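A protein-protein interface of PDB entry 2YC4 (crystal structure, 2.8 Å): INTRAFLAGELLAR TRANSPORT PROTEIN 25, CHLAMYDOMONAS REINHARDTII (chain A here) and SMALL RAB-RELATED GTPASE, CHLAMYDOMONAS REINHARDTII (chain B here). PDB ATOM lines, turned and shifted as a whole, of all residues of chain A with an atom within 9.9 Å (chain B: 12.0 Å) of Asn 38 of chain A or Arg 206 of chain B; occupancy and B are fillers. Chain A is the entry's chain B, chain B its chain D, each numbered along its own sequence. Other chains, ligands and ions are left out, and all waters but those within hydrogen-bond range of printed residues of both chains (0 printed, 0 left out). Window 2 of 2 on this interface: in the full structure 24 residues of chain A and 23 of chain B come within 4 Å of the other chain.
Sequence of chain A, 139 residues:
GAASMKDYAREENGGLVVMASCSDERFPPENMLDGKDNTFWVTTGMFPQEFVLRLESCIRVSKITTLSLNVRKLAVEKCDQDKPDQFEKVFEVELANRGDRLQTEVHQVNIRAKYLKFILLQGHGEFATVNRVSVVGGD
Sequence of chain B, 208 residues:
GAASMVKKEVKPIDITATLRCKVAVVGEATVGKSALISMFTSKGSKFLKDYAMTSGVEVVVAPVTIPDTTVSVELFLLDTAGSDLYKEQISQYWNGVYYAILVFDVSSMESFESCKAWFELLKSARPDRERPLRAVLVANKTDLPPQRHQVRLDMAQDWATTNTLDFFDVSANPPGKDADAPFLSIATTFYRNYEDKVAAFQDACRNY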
ATOM      1  N   ARG A  26     -13.100   9.530  -4.110  1.00  0.00           N
ATOM      2  CA  ARG A  26     -11.978   9.475  -5.042  1.00  0.00           C
ATOM      3  C   ARG A  26     -12.356   9.916  -6.429  1.00  0.00           C
ATOM      4  O   ARG A  26     -11.483  10.120  -7.268  1.00  0.00           O
ATOM      5  CB  ARG A  26     -11.411   8.061  -5.147  1.00  0.00           C
ATOM      6  CG  ARG A  26     -10.442   7.684  -4.069  1.00  0.00           C
ATOM      7  CD  ARG A  26      -9.985   6.280  -4.315  1.00  0.00           C
ATOM      8  NE  ARG A  26     -11.113   5.360  -4.336  1.00  0.00           N
ATOM      9  CZ  ARG A  26     -10.993   4.042  -4.471  1.00  0.00           C
ATOM     10  NH1 ARG A  26      -9.778   3.505  -4.597  1.00  0.00           N
ATOM     11  NH2 ARG A  26     -12.080   3.263  -4.478  1.00  0.00           N
ATOM     12  N   PHE A  27     -13.658  10.022  -6.680  1.00  0.00           N
ATOM     13  CA  PHE A  27     -14.175  10.310  -8.018  1.00  0.00           C
ATOM     14  C   PHE A  27     -15.467  11.025  -7.839  1.00  0.00           C
ATOM     15  O   PHE A  27     -16.510  10.510  -8.208  1.00  0.00           O
ATOM     16  CB  PHE A  27     -14.415   9.016  -8.780  1.00  0.00           C
ATOM     17  CG  PHE A  27     -13.302   8.021  -8.627  1.00  0.00           C
ATOM     18  CD1 PHE A  27     -12.172   8.101  -9.420  1.00  0.00           C
ATOM     19  CD2 PHE A  27     -13.373   7.020  -7.671  1.00  0.00           C
ATOM     20  CE1 PHE A  27     -11.155   7.200  -9.283  1.00  0.00           C
ATOM     21  CE2 PHE A  27     -12.346   6.120  -7.515  1.00  0.00           C
ATOM     22  CZ  PHE A  27     -11.241   6.205  -8.323  1.00  0.00           C
ATOM     23  N   ASN A  31     -15.773  16.120 -10.588  1.00  0.00           N
ATOM     24  CA  ASN A  31     -14.925  15.690 -11.687  1.00  0.00           C
ATOM     25  C   ASN A  31     -15.605  15.739 -13.039  1.00  0.00           C
ATOM     26  O   ASN A  31     -15.017  15.344 -14.049  1.00  0.00           O
ATOM     27  CB  ASN A  31     -14.432  14.267 -11.455  1.00  0.00           C
ATOM     28  CG  ASN A  31     -13.226  14.198 -10.522  1.00  0.00           C
ATOM     29  OD1 ASN A  31     -12.639  13.126 -10.343  1.00  0.00           O
ATOM     30  ND2 ASN A  31     -12.860  15.338  -9.910  1.00  0.00           N
ATOM     31  N   MET A  32     -16.853  16.192 -13.067  1.00  0.00           N
ATOM     32  CA  MET A  32     -17.601  16.201 -14.323  1.00  0.00           C
ATOM     33  C   MET A  32     -17.527  17.565 -14.982  1.00  0.00           C
ATOM     34  O   MET A  32     -17.703  17.691 -16.191  1.00  0.00           O
ATOM     35  CB  MET A  32     -19.059  15.757 -14.110  1.00  0.00           C
ATOM     36  CG  MET A  32     -19.171  14.311 -13.652  1.00  0.00           C
ATOM     37  SD  MET A  32     -20.838  13.639 -13.491  1.00  0.00           S
ATOM     38  CE  MET A  32     -21.269  14.071 -11.802  1.00  0.00           C
ATOM     39  N   ASP A  34     -14.853  19.988 -14.448  1.00  0.00           N
ATOM     40  CA  ASP A  34     -13.555  20.646 -14.410  1.00  0.00           C
ATOM     41  C   ASP A  34     -12.986  20.781 -15.823  1.00  0.00           C
ATOM     42  O   ASP A  34     -11.913  21.345 -16.011  1.00  0.00           O
ATOM     43  CB  ASP A  34     -12.589  19.910 -13.478  1.00  0.00           C
ATOM     44  CG  ASP A  34     -12.462  18.425 -13.812  1.00  0.00           C
ATOM     45  OD1 ASP A  34     -12.720  18.047 -14.983  1.00  0.00           O
ATOM     46  OD2 ASP A  34     -12.095  17.642 -12.900  1.00  0.00           O
ATOM     47  N   GLY A  35     -13.704  20.260 -16.815  1.00  0.00           N
ATOM     48  CA  GLY A  35     -13.312  20.451 -18.199  1.00  0.00           C
ATOM     49  C   GLY A  35     -12.194  19.542 -18.675  1.00  0.00           C
ATOM     50  O   GLY A  35     -11.823  19.566 -19.855  1.00  0.00           O
ATOM     51  N   LYS A  36     -11.655  18.737 -17.765  1.00  0.00           N
ATOM     52  CA  LYS A  36     -10.628  17.758 -18.117  1.00  0.00           C
ATOM     53  C   LYS A  36     -11.294  16.486 -18.633  1.00  0.00           C
ATOM     54  O   LYS A  36     -12.457  16.227 -18.343  1.00  0.00           O
ATOM     55  CB  LYS A  36      -9.738  17.456 -16.910  1.00  0.00           C
ATOM     56  N   ASP A  37     -10.579  15.695 -19.413  1.00  0.00           N
ATOM     57  CA  ASP A  37     -11.193  14.498 -19.959  1.00  0.00           C
ATOM     58  C   ASP A  37     -10.736  13.273 -19.198  1.00  0.00           C
ATOM     59  O   ASP A  37     -11.242  12.179 -19.424  1.00  0.00           O
ATOM     60  CB  ASP A  37     -10.848  14.341 -21.436  1.00  0.00           C
ATOM     61  CG  ASP A  37     -11.958  14.820 -22.341  1.00  0.00           C
ATOM     62  OD1 ASP A  37     -12.843  15.534 -21.833  1.00  0.00           O
ATOM     63  OD2 ASP A  37     -11.950  14.490 -23.554  1.00  0.00           O
ATOM     64  N   ASN A  38      -9.774  13.451 -18.300  1.00  0.00           N
ATOM     65  CA  ASN A  38      -9.127  12.306 -17.662  1.00  0.00           C
ATOM     66  C   ASN A  38      -9.631  12.047 -16.256  1.00  0.00           C
ATOM     67  O   ASN A  38      -9.330  11.017 -15.661  1.00  0.00           O
ATOM     68  CB  ASN A  38      -7.604  12.455 -17.659  1.00  0.00           C
ATOM     69  CG  ASN A  38      -7.136  13.620 -16.811  1.00  0.00           C
ATOM     70  OD1 ASN A  38      -6.665  13.435 -15.693  1.00  0.00           O
ATOM     71  ND2 ASN A  38      -7.267  14.831 -17.343  1.00  0.00           N
ATOM     72  N   THR A  39     -10.393  12.989 -15.722  1.00  0.00           N
ATOM     73  CA  THR A  39     -11.032  12.779 -14.433  1.00  0.00           C
ATOM     74  C   THR A  39     -12.497  12.402 -14.672  1.00  0.00           C
ATOM     75  O   THR A  39     -13.038  12.642 -15.757  1.00  0.00           O
ATOM     76  CB  THR A  39     -10.859  14.007 -13.494  1.00  0.00           C
ATOM     77  OG1 THR A  39     -11.173  15.221 -14.193  1.00  0.00           O
ATOM     78  CG2 THR A  39      -9.420  14.095 -13.041  1.00  0.00           C
ATOM     79  N   PHE A  40     -13.131  11.777 -13.684  1.00  0.00           N
ATOM     80  CA  PHE A  40     -14.509  11.343 -13.859  1.00  0.00           C
ATOM     81  C   PHE A  40     -15.231  11.130 -12.551  1.00  0.00           C
ATOM     82  O   PHE A  40     -14.643  11.174 -11.468  1.00  0.00           O
ATOM     83  CB  PHE A  40     -14.566  10.038 -14.640  1.00  0.00           C
ATOM     84  CG  PHE A  40     -13.844   8.915 -13.970  1.00  0.00           C
ATOM     85  CD1 PHE A  40     -12.486   8.723 -14.172  1.00  0.00           C
ATOM     86  CD2 PHE A  40     -14.509   8.050 -13.128  1.00  0.00           C
ATOM     87  CE1 PHE A  40     -11.805   7.688 -13.555  1.00  0.00           C
ATOM     88  CE2 PHE A  40     -13.830   7.007 -12.511  1.00  0.00           C
ATOM     89  CZ  PHE A  40     -12.477   6.834 -12.726  1.00  0.00           C
ATOM     90  N   TRP A  41     -16.528  10.906 -12.688  1.00  0.00           N
ATOM     91  CA  TRP A  41     -17.372  10.443 -11.613  1.00  0.00           C
ATOM     92  C   TRP A  41     -17.734   9.005 -11.958  1.00  0.00           C
ATOM     93  O   TRP A  41     -17.985   8.685 -13.124  1.00  0.00           O
ATOM     94  CB  TRP A  41     -18.617  11.307 -11.533  1.00  0.00           C
ATOM     95  CG  TRP A  41     -19.659  10.811 -10.607  1.00  0.00           C
ATOM     96  CD1 TRP A  41     -19.632  10.856  -9.249  1.00  0.00           C
ATOM     97  CD2 TRP A  41     -20.915  10.224 -10.967  1.00  0.00           C
ATOM     98  NE1 TRP A  41     -20.792  10.324  -8.728  1.00  0.00           N
ATOM     99  CE2 TRP A  41     -21.599   9.927  -9.763  1.00  0.00           C
ATOM    100  CE3 TRP A  41     -21.527   9.908 -12.187  1.00  0.00           C
ATOM    101  CZ2 TRP A  41     -22.861   9.332  -9.746  1.00  0.00           C
ATOM    102  CZ3 TRP A  41     -22.782   9.313 -12.164  1.00  0.00           C
ATOM    103  CH2 TRP A  41     -23.433   9.037 -10.949  1.00  0.00           C
ATOM    104  N   LEU A  67     -19.532  13.102 -21.736  1.00  0.00           N
ATOM    105  CA  LEU A  67     -18.405  12.217 -21.980  1.00  0.00           C
ATOM    106  C   LEU A  67     -18.427  11.137 -20.930  1.00  0.00           C
ATOM    107  O   LEU A  67     -18.294  11.425 -19.748  1.00  0.00           O
ATOM    108  CB  LEU A  67     -17.102  12.985 -21.845  1.00  0.00           C
ATOM    109  CG  LEU A  67     -16.149  12.854 -23.023  1.00  0.00           C
ATOM    110  CD1 LEU A  67     -15.828  11.381 -23.248  1.00  0.00           C
ATOM    111  CD2 LEU A  67     -16.764  13.487 -24.279  1.00  0.00           C
ATOM    112  N   LEU A  69     -18.130   6.598 -19.855  1.00  0.00           N
ATOM    113  CA  LEU A  69     -17.622   5.245 -20.080  1.00  0.00           C
ATOM    114  C   LEU A  69     -18.620   4.214 -19.566  1.00  0.00           C
ATOM    115  O   LEU A  69     -19.028   4.268 -18.416  1.00  0.00           O
ATOM    116  CB  LEU A  69     -16.294   5.052 -19.342  1.00  0.00           C
ATOM    117  CG  LEU A  69     -15.022   4.694 -20.107  1.00  0.00           C
ATOM    118  CD1 LEU A  69     -13.856   5.495 -19.542  1.00  0.00           C
ATOM    119  CD2 LEU A  69     -14.743   3.178 -20.039  1.00  0.00           C
ATOM    120  N   GLY A  99     -14.816   0.850 -24.345  1.00  0.00           N
ATOM    121  CA  GLY A  99     -14.206   1.463 -23.175  1.00  0.00           C
ATOM    122  C   GLY A  99     -13.684   2.829 -23.598  1.00  0.00           C
ATOM    123  O   GLY A  99     -12.825   3.400 -22.939  1.00  0.00           O
ATOM    124  N   LEU A 102     -14.391   5.502 -24.484  1.00  0.00           N
ATOM    125  CA  LEU A 102     -15.178   6.687 -24.130  1.00  0.00           C
ATOM    126  C   LEU A 102     -16.317   6.991 -25.105  1.00  0.00           C
ATOM    127  O   LEU A 102     -16.187   6.852 -26.332  1.00  0.00           O
ATOM    128  CB  LEU A 102     -14.283   7.938 -23.938  1.00  0.00           C
ATOM    129  N   THR A 129     -18.936   5.534 -15.762  1.00  0.00           N
ATOM    130  CA  THR A 129     -18.307   6.799 -15.398  1.00  0.00           C
ATOM    131  C   THR A 129     -18.842   7.947 -16.217  1.00  0.00           C
ATOM    132  O   THR A 129     -19.268   7.770 -17.358  1.00  0.00           O
ATOM    133  CB  THR A 129     -16.771   6.784 -15.585  1.00  0.00           C
ATOM    134  OG1 THR A 129     -16.455   6.762 -16.976  1.00  0.00           O
ATOM    135  CG2 THR A 129     -16.136   5.588 -14.928  1.00  0.00           C
ATOM    136  N   VAL A 130     -18.824   9.132 -15.622  1.00  0.00           N
ATOM    137  CA  VAL A 130     -19.022  10.339 -16.385  1.00  0.00           C
ATOM    138  C   VAL A 130     -17.814  11.233 -16.158  1.00  0.00           C
ATOM    139  O   VAL A 130     -17.424  11.511 -15.040  1.00  0.00           O
ATOM    140  CB  VAL A 130     -20.345  11.040 -16.039  1.00  0.00           C
ATOM    141  CG1 VAL A 130     -20.596  12.206 -17.026  1.00  0.00           C
ATOM    142  CG2 VAL A 130     -21.473  10.053 -16.114  1.00  0.00           C
ATOM    143  N   ASN A 131     -17.208  11.660 -17.248  1.00  0.00           N
ATOM    144  CA  ASN A 131     -15.933  12.345 -17.195  1.00  0.00           C
ATOM    145  C   ASN A 131     -16.146  13.825 -17.424  1.00  0.00           C
ATOM    146  O   ASN A 131     -15.673  14.664 -16.651  1.00  0.00           O
ATOM    147  CB  ASN A 131     -15.020  11.783 -18.275  1.00  0.00           C
ATOM    148  CG  ASN A 131     -14.946  10.273 -18.244  1.00  0.00           C
ATOM    149  OD1 ASN A 131     -15.835   9.573 -18.739  1.00  0.00           O
ATOM    150  ND2 ASN A 131     -13.876   9.758 -17.655  1.00  0.00           N
ATOM    151  N   ARG A 132     -16.879  14.142 -18.487  1.00  0.00           N
ATOM    152  CA  ARG A 132     -17.304  15.517 -18.700  1.00  0.00           C
ATOM    153  C   ARG A 132     -18.811  15.682 -18.879  1.00  0.00           C
ATOM    154  O   ARG A 132     -19.487  14.853 -19.508  1.00  0.00           O
ATOM    155  CB  ARG A 132     -16.587  16.125 -19.893  1.00  0.00           C
ATOM    156  CG  ARG A 132     -15.105  16.276 -19.700  1.00  0.00           C
ATOM    157  CD  ARG A 132     -14.588  17.413 -20.560  1.00  0.00           C
ATOM    158  NE  ARG A 132     -15.235  18.675 -20.216  1.00  0.00           N
ATOM    159  CZ  ARG A 132     -16.104  19.297 -21.000  1.00  0.00           C
ATOM    160  NH1 ARG A 132     -16.425  18.765 -22.173  1.00  0.00           N
ATOM    161  NH2 ARG A 132     -16.651  20.444 -20.608  1.00  0.00           N
ATOM    162  N   LYS B 197     -12.370  -2.622 -11.526  1.00  0.00           N
ATOM    163  CA  LYS B 197     -13.005  -1.876 -12.604  1.00  0.00           C
ATOM    164  C   LYS B 197     -12.619  -0.407 -12.560  1.00  0.00           C
ATOM    165  O   LYS B 197     -12.348   0.209 -13.593  1.00  0.00           O
ATOM    166  CB  LYS B 197     -14.531  -2.010 -12.527  1.00  0.00           C
ATOM    167  CG  LYS B 197     -15.051  -3.431 -12.597  1.00  0.00           C
ATOM    168  CD  LYS B 197     -14.636  -4.118 -13.877  1.00  0.00           C
ATOM    169  CE  LYS B 197     -15.089  -5.570 -13.902  1.00  0.00           C
ATOM    170  NZ  LYS B 197     -16.574  -5.725 -13.638  1.00  0.00           N
ATOM    171  N   VAL B 198     -12.616   0.147 -11.355  1.00  0.00           N
ATOM    172  CA  VAL B 198     -12.249   1.540 -11.136  1.00  0.00           C
ATOM    173  C   VAL B 198     -10.828   1.867 -11.601  1.00  0.00           C
ATOM    174  O   VAL B 198     -10.573   2.961 -12.101  1.00  0.00           O
ATOM    175  CB  VAL B 198     -12.382   1.912  -9.647  1.00  0.00           C
ATOM    176  CG1 VAL B 198     -11.952   3.332  -9.412  1.00  0.00           C
ATOM    177  CG2 VAL B 198     -13.804   1.734  -9.197  1.00  0.00           C
ATOM    178  N   ALA B 199      -9.900   0.932 -11.418  1.00  0.00           N
ATOM    179  CA  ALA B 199      -8.533   1.152 -11.842  1.00  0.00           C
ATOM    180  C   ALA B 199      -8.474   1.039 -13.354  1.00  0.00           C
ATOM    181  O   ALA B 199      -7.856   1.859 -14.039  1.00  0.00           O
ATOM    182  CB  ALA B 199      -7.638   0.145 -11.195  1.00  0.00           C
ATOM    183  N   ALA B 200      -9.131   0.012 -13.864  1.00  0.00           N
ATOM    184  CA  ALA B 200      -9.317  -0.145 -15.292  1.00  0.00           C
ATOM    185  C   ALA B 200      -9.786   1.157 -15.928  1.00  0.00           C
ATOM    186  O   ALA B 200      -9.300   1.537 -16.985  1.00  0.00           O
ATOM    187  CB  ALA B 200     -10.316  -1.251 -15.572  1.00  0.00           C
ATOM    188  N   PHE B 201     -10.733   1.838 -15.295  1.00  0.00           N
ATOM    189  CA  PHE B 201     -11.217   3.106 -15.821  1.00  0.00           C
ATOM    190  C   PHE B 201     -10.134   4.172 -15.847  1.00  0.00           C
ATOM    191  O   PHE B 201      -9.983   4.870 -16.827  1.00  0.00           O
ATOM    192  CB  PHE B 201     -12.409   3.621 -15.015  1.00  0.00           C
ATOM    193  CG  PHE B 201     -13.673   2.843 -15.242  1.00  0.00           C
ATOM    194  CD1 PHE B 201     -13.875   2.143 -16.422  1.00  0.00           C
ATOM    195  CD2 PHE B 201     -14.657   2.788 -14.270  1.00  0.00           C
ATOM    196  CE1 PHE B 201     -15.050   1.413 -16.624  1.00  0.00           C
ATOM    197  CE2 PHE B 201     -15.829   2.060 -14.474  1.00  0.00           C
ATOM    198  CZ  PHE B 201     -16.024   1.379 -15.647  1.00  0.00           C
ATOM    199  N   GLN B 202      -9.390   4.314 -14.764  1.00  0.00           N
ATOM    200  CA  GLN B 202      -8.319   5.296 -14.720  1.00  0.00           C
ATOM    201  C   GLN B 202      -7.300   5.014 -15.808  1.00  0.00           C
ATOM    202  O   GLN B 202      -6.699   5.934 -16.351  1.00  0.00           O
ATOM    203  CB  GLN B 202      -7.650   5.274 -13.357  1.00  0.00           C
ATOM    204  CG  GLN B 202      -8.613   5.522 -12.248  1.00  0.00           C
ATOM    205  CD  GLN B 202      -7.926   5.711 -10.916  1.00  0.00           C
ATOM    206  OE1 GLN B 202      -7.642   4.733 -10.215  1.00  0.00           O
ATOM    207  NE2 GLN B 202      -7.661   6.971 -10.549  1.00  0.00           N
ATOM    208  N   ASP B 203      -7.111   3.729 -16.100  1.00  0.00           N
ATOM    209  CA  ASP B 203      -6.254   3.263 -17.182  1.00  0.00           C
ATOM    210  C   ASP B 203      -6.726   3.769 -18.526  1.00  0.00           C
ATOM    211  O   ASP B 203      -5.938   4.148 -19.379  1.00  0.00           O
ATOM    212  CB  ASP B 203      -6.333   1.745 -17.254  1.00  0.00           C
ATOM    213  CG  ASP B 203      -5.079   1.079 -16.785  1.00  0.00           C
ATOM    214  OD1 ASP B 203      -4.089   1.810 -16.549  1.00  0.00           O
ATOM    215  OD2 ASP B 203      -5.081  -0.171 -16.669  1.00  0.00           O
ATOM    216  N   ALA B 204      -8.035   3.729 -18.714  1.00  0.00           N
ATOM    217  CA  ALA B 204      -8.617   3.893 -20.023  1.00  0.00           C
ATOM    218  C   ALA B 204      -8.779   5.357 -20.406  1.00  0.00           C
ATOM    219  O   ALA B 204      -9.138   5.661 -21.539  1.00  0.00           O
ATOM    220  CB  ALA B 204      -9.948   3.164 -20.097  1.00  0.00           C
ATOM    221  N   CYS B 205      -8.488   6.271 -19.493  1.00  0.00           N
ATOM    222  CA  CYS B 205      -8.815   7.660 -19.781  1.00  0.00           C
ATOM    223  C   CYS B 205      -7.699   8.709 -19.558  1.00  0.00           C
ATOM    224  O   CYS B 205      -7.986   9.902 -19.448  1.00  0.00           O
ATOM    225  CB  CYS B 205     -10.113   8.065 -19.050  1.00  0.00           C
ATOM    226  SG  CYS B 205      -9.963   8.347 -17.254  1.00  0.00           S
ATOM    227  N   ARG B 206      -6.427   8.328 -19.536  1.00  0.00           N
ATOM    228  CA  ARG B 206      -5.421   9.385 -19.365  1.00  0.00           C
ATOM    229  C   ARG B 206      -4.616   9.688 -20.645  1.00  0.00           C
ATOM    230  O   ARG B 206      -3.782   8.871 -21.050  1.00  0.00           O
ATOM    231  CB  ARG B 206      -4.501   9.070 -18.181  1.00  0.00           C
ATOM    232  CG  ARG B 206      -3.291   9.990 -18.058  1.00  0.00           C
ATOM    233  CD  ARG B 206      -3.643  11.419 -17.656  1.00  0.00           C
ATOM    234  NE  ARG B 206      -2.434  12.233 -17.504  1.00  0.00           N
ATOM    235  CZ  ARG B 206      -2.241  13.150 -16.554  1.00  0.00           C
ATOM    236  NH1 ARG B 206      -3.186  13.388 -15.650  1.00  0.00           N
ATOM    237  NH2 ARG B 206      -1.099  13.835 -16.506  1.00  0.00           N
ATOM    238  N   ASN B 207      -4.860  10.836 -21.295  1.00  0.00           N
ATOM    239  CA  ASN B 207      -5.843  11.849 -20.881  1.00  0.00           C
ATOM    240  C   ASN B 207      -7.024  12.034 -21.860  1.00  0.00           C
ATOM    241  O   ASN B 207      -7.200  11.279 -22.825  1.00  0.00           O
ATOM    242  CB  ASN B 207      -5.150  13.190 -20.651  1.00  0.00           C
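The side-chain amide oxygen of Asn 31 of chain A sits close to the backbone carbonyl oxygen of Phe 40 of chain A (3.0 Å). The backbone carbonyl oxygen (O) of Leu 69 of chain A sits at hydrogen-bond distance from the backbone NH (N) of Thr 129 of chain A, 2.9 Å away. The side-chain amide oxygen (OD1) of Asn 131 of chain A sits at hydrogen-bond distance from the side-chain hydroxyl (OG1) of Thr 129 of chain A, at 3.4 Å. The backbone carbonyl oxygen of Phe 201 of chain B is in hydrogen-bond range of the side-chain sulfur of Cys 205 of chain B (3.5 Å).
Among the printed residues, merely in contact across the chains: Phe 27 of chain A with Val 198 of chain B (3.2 Å), Phe 27 of chain A with Gln 202 of chain B (3.7 Å), Asp 37 of chain A with Cys 205 of chain B (3.97 Å), Asn 38 of chain A with Asn 207 of chain B (3.7 Å), Phe 40 of chain A with Phe 201 of chain B (3.9 Å), Leu 69 of chain A with Phe 201 of chain B (3.9 Å) and Thr 129 of chain A with Phe 201 of chain B (3.2 Å).
Asn 38 of chain A touches three residues of chain B. Arg 206 of chain B touches just one residue of chain A: Asn 38. Printed residues of chain B within 4 Å of Asp 37 of chain A: Cys 205 (3.97 Å). No residue of chain B comes within 4 Å of Thr 39 of chain A. No residue of chain B comes within 4 Å of Asn 131 of chain A. Asn 207 of chain B touches one residue of chain A. Of the printed residues of chain A, Cys 205 of chain B touches Asp 37 and Asn 38. Of the printed residues of chain B, Leu 69 of chain A touches Phe 201.
Printed residues of chain A that touch a printed residue of chain B: Phe 27, Asp 37, Asn 38, Phe 40, Leu 69 and Thr 129. Hydrophobic or aromatic side chains of chain B that line the printed part of chain A: Val 198 and Phe 201.
The backbone carbonyl oxygen of Asn 38 of chain A is in hydrogen-bond range of the side-chain sulfur of Cys 205 of chain B (3.2 Å). OD1 of Asn 38 of chain A lies within hydrogen-bond range of NH1 of Arg 206 of chain B (3.5 Å).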
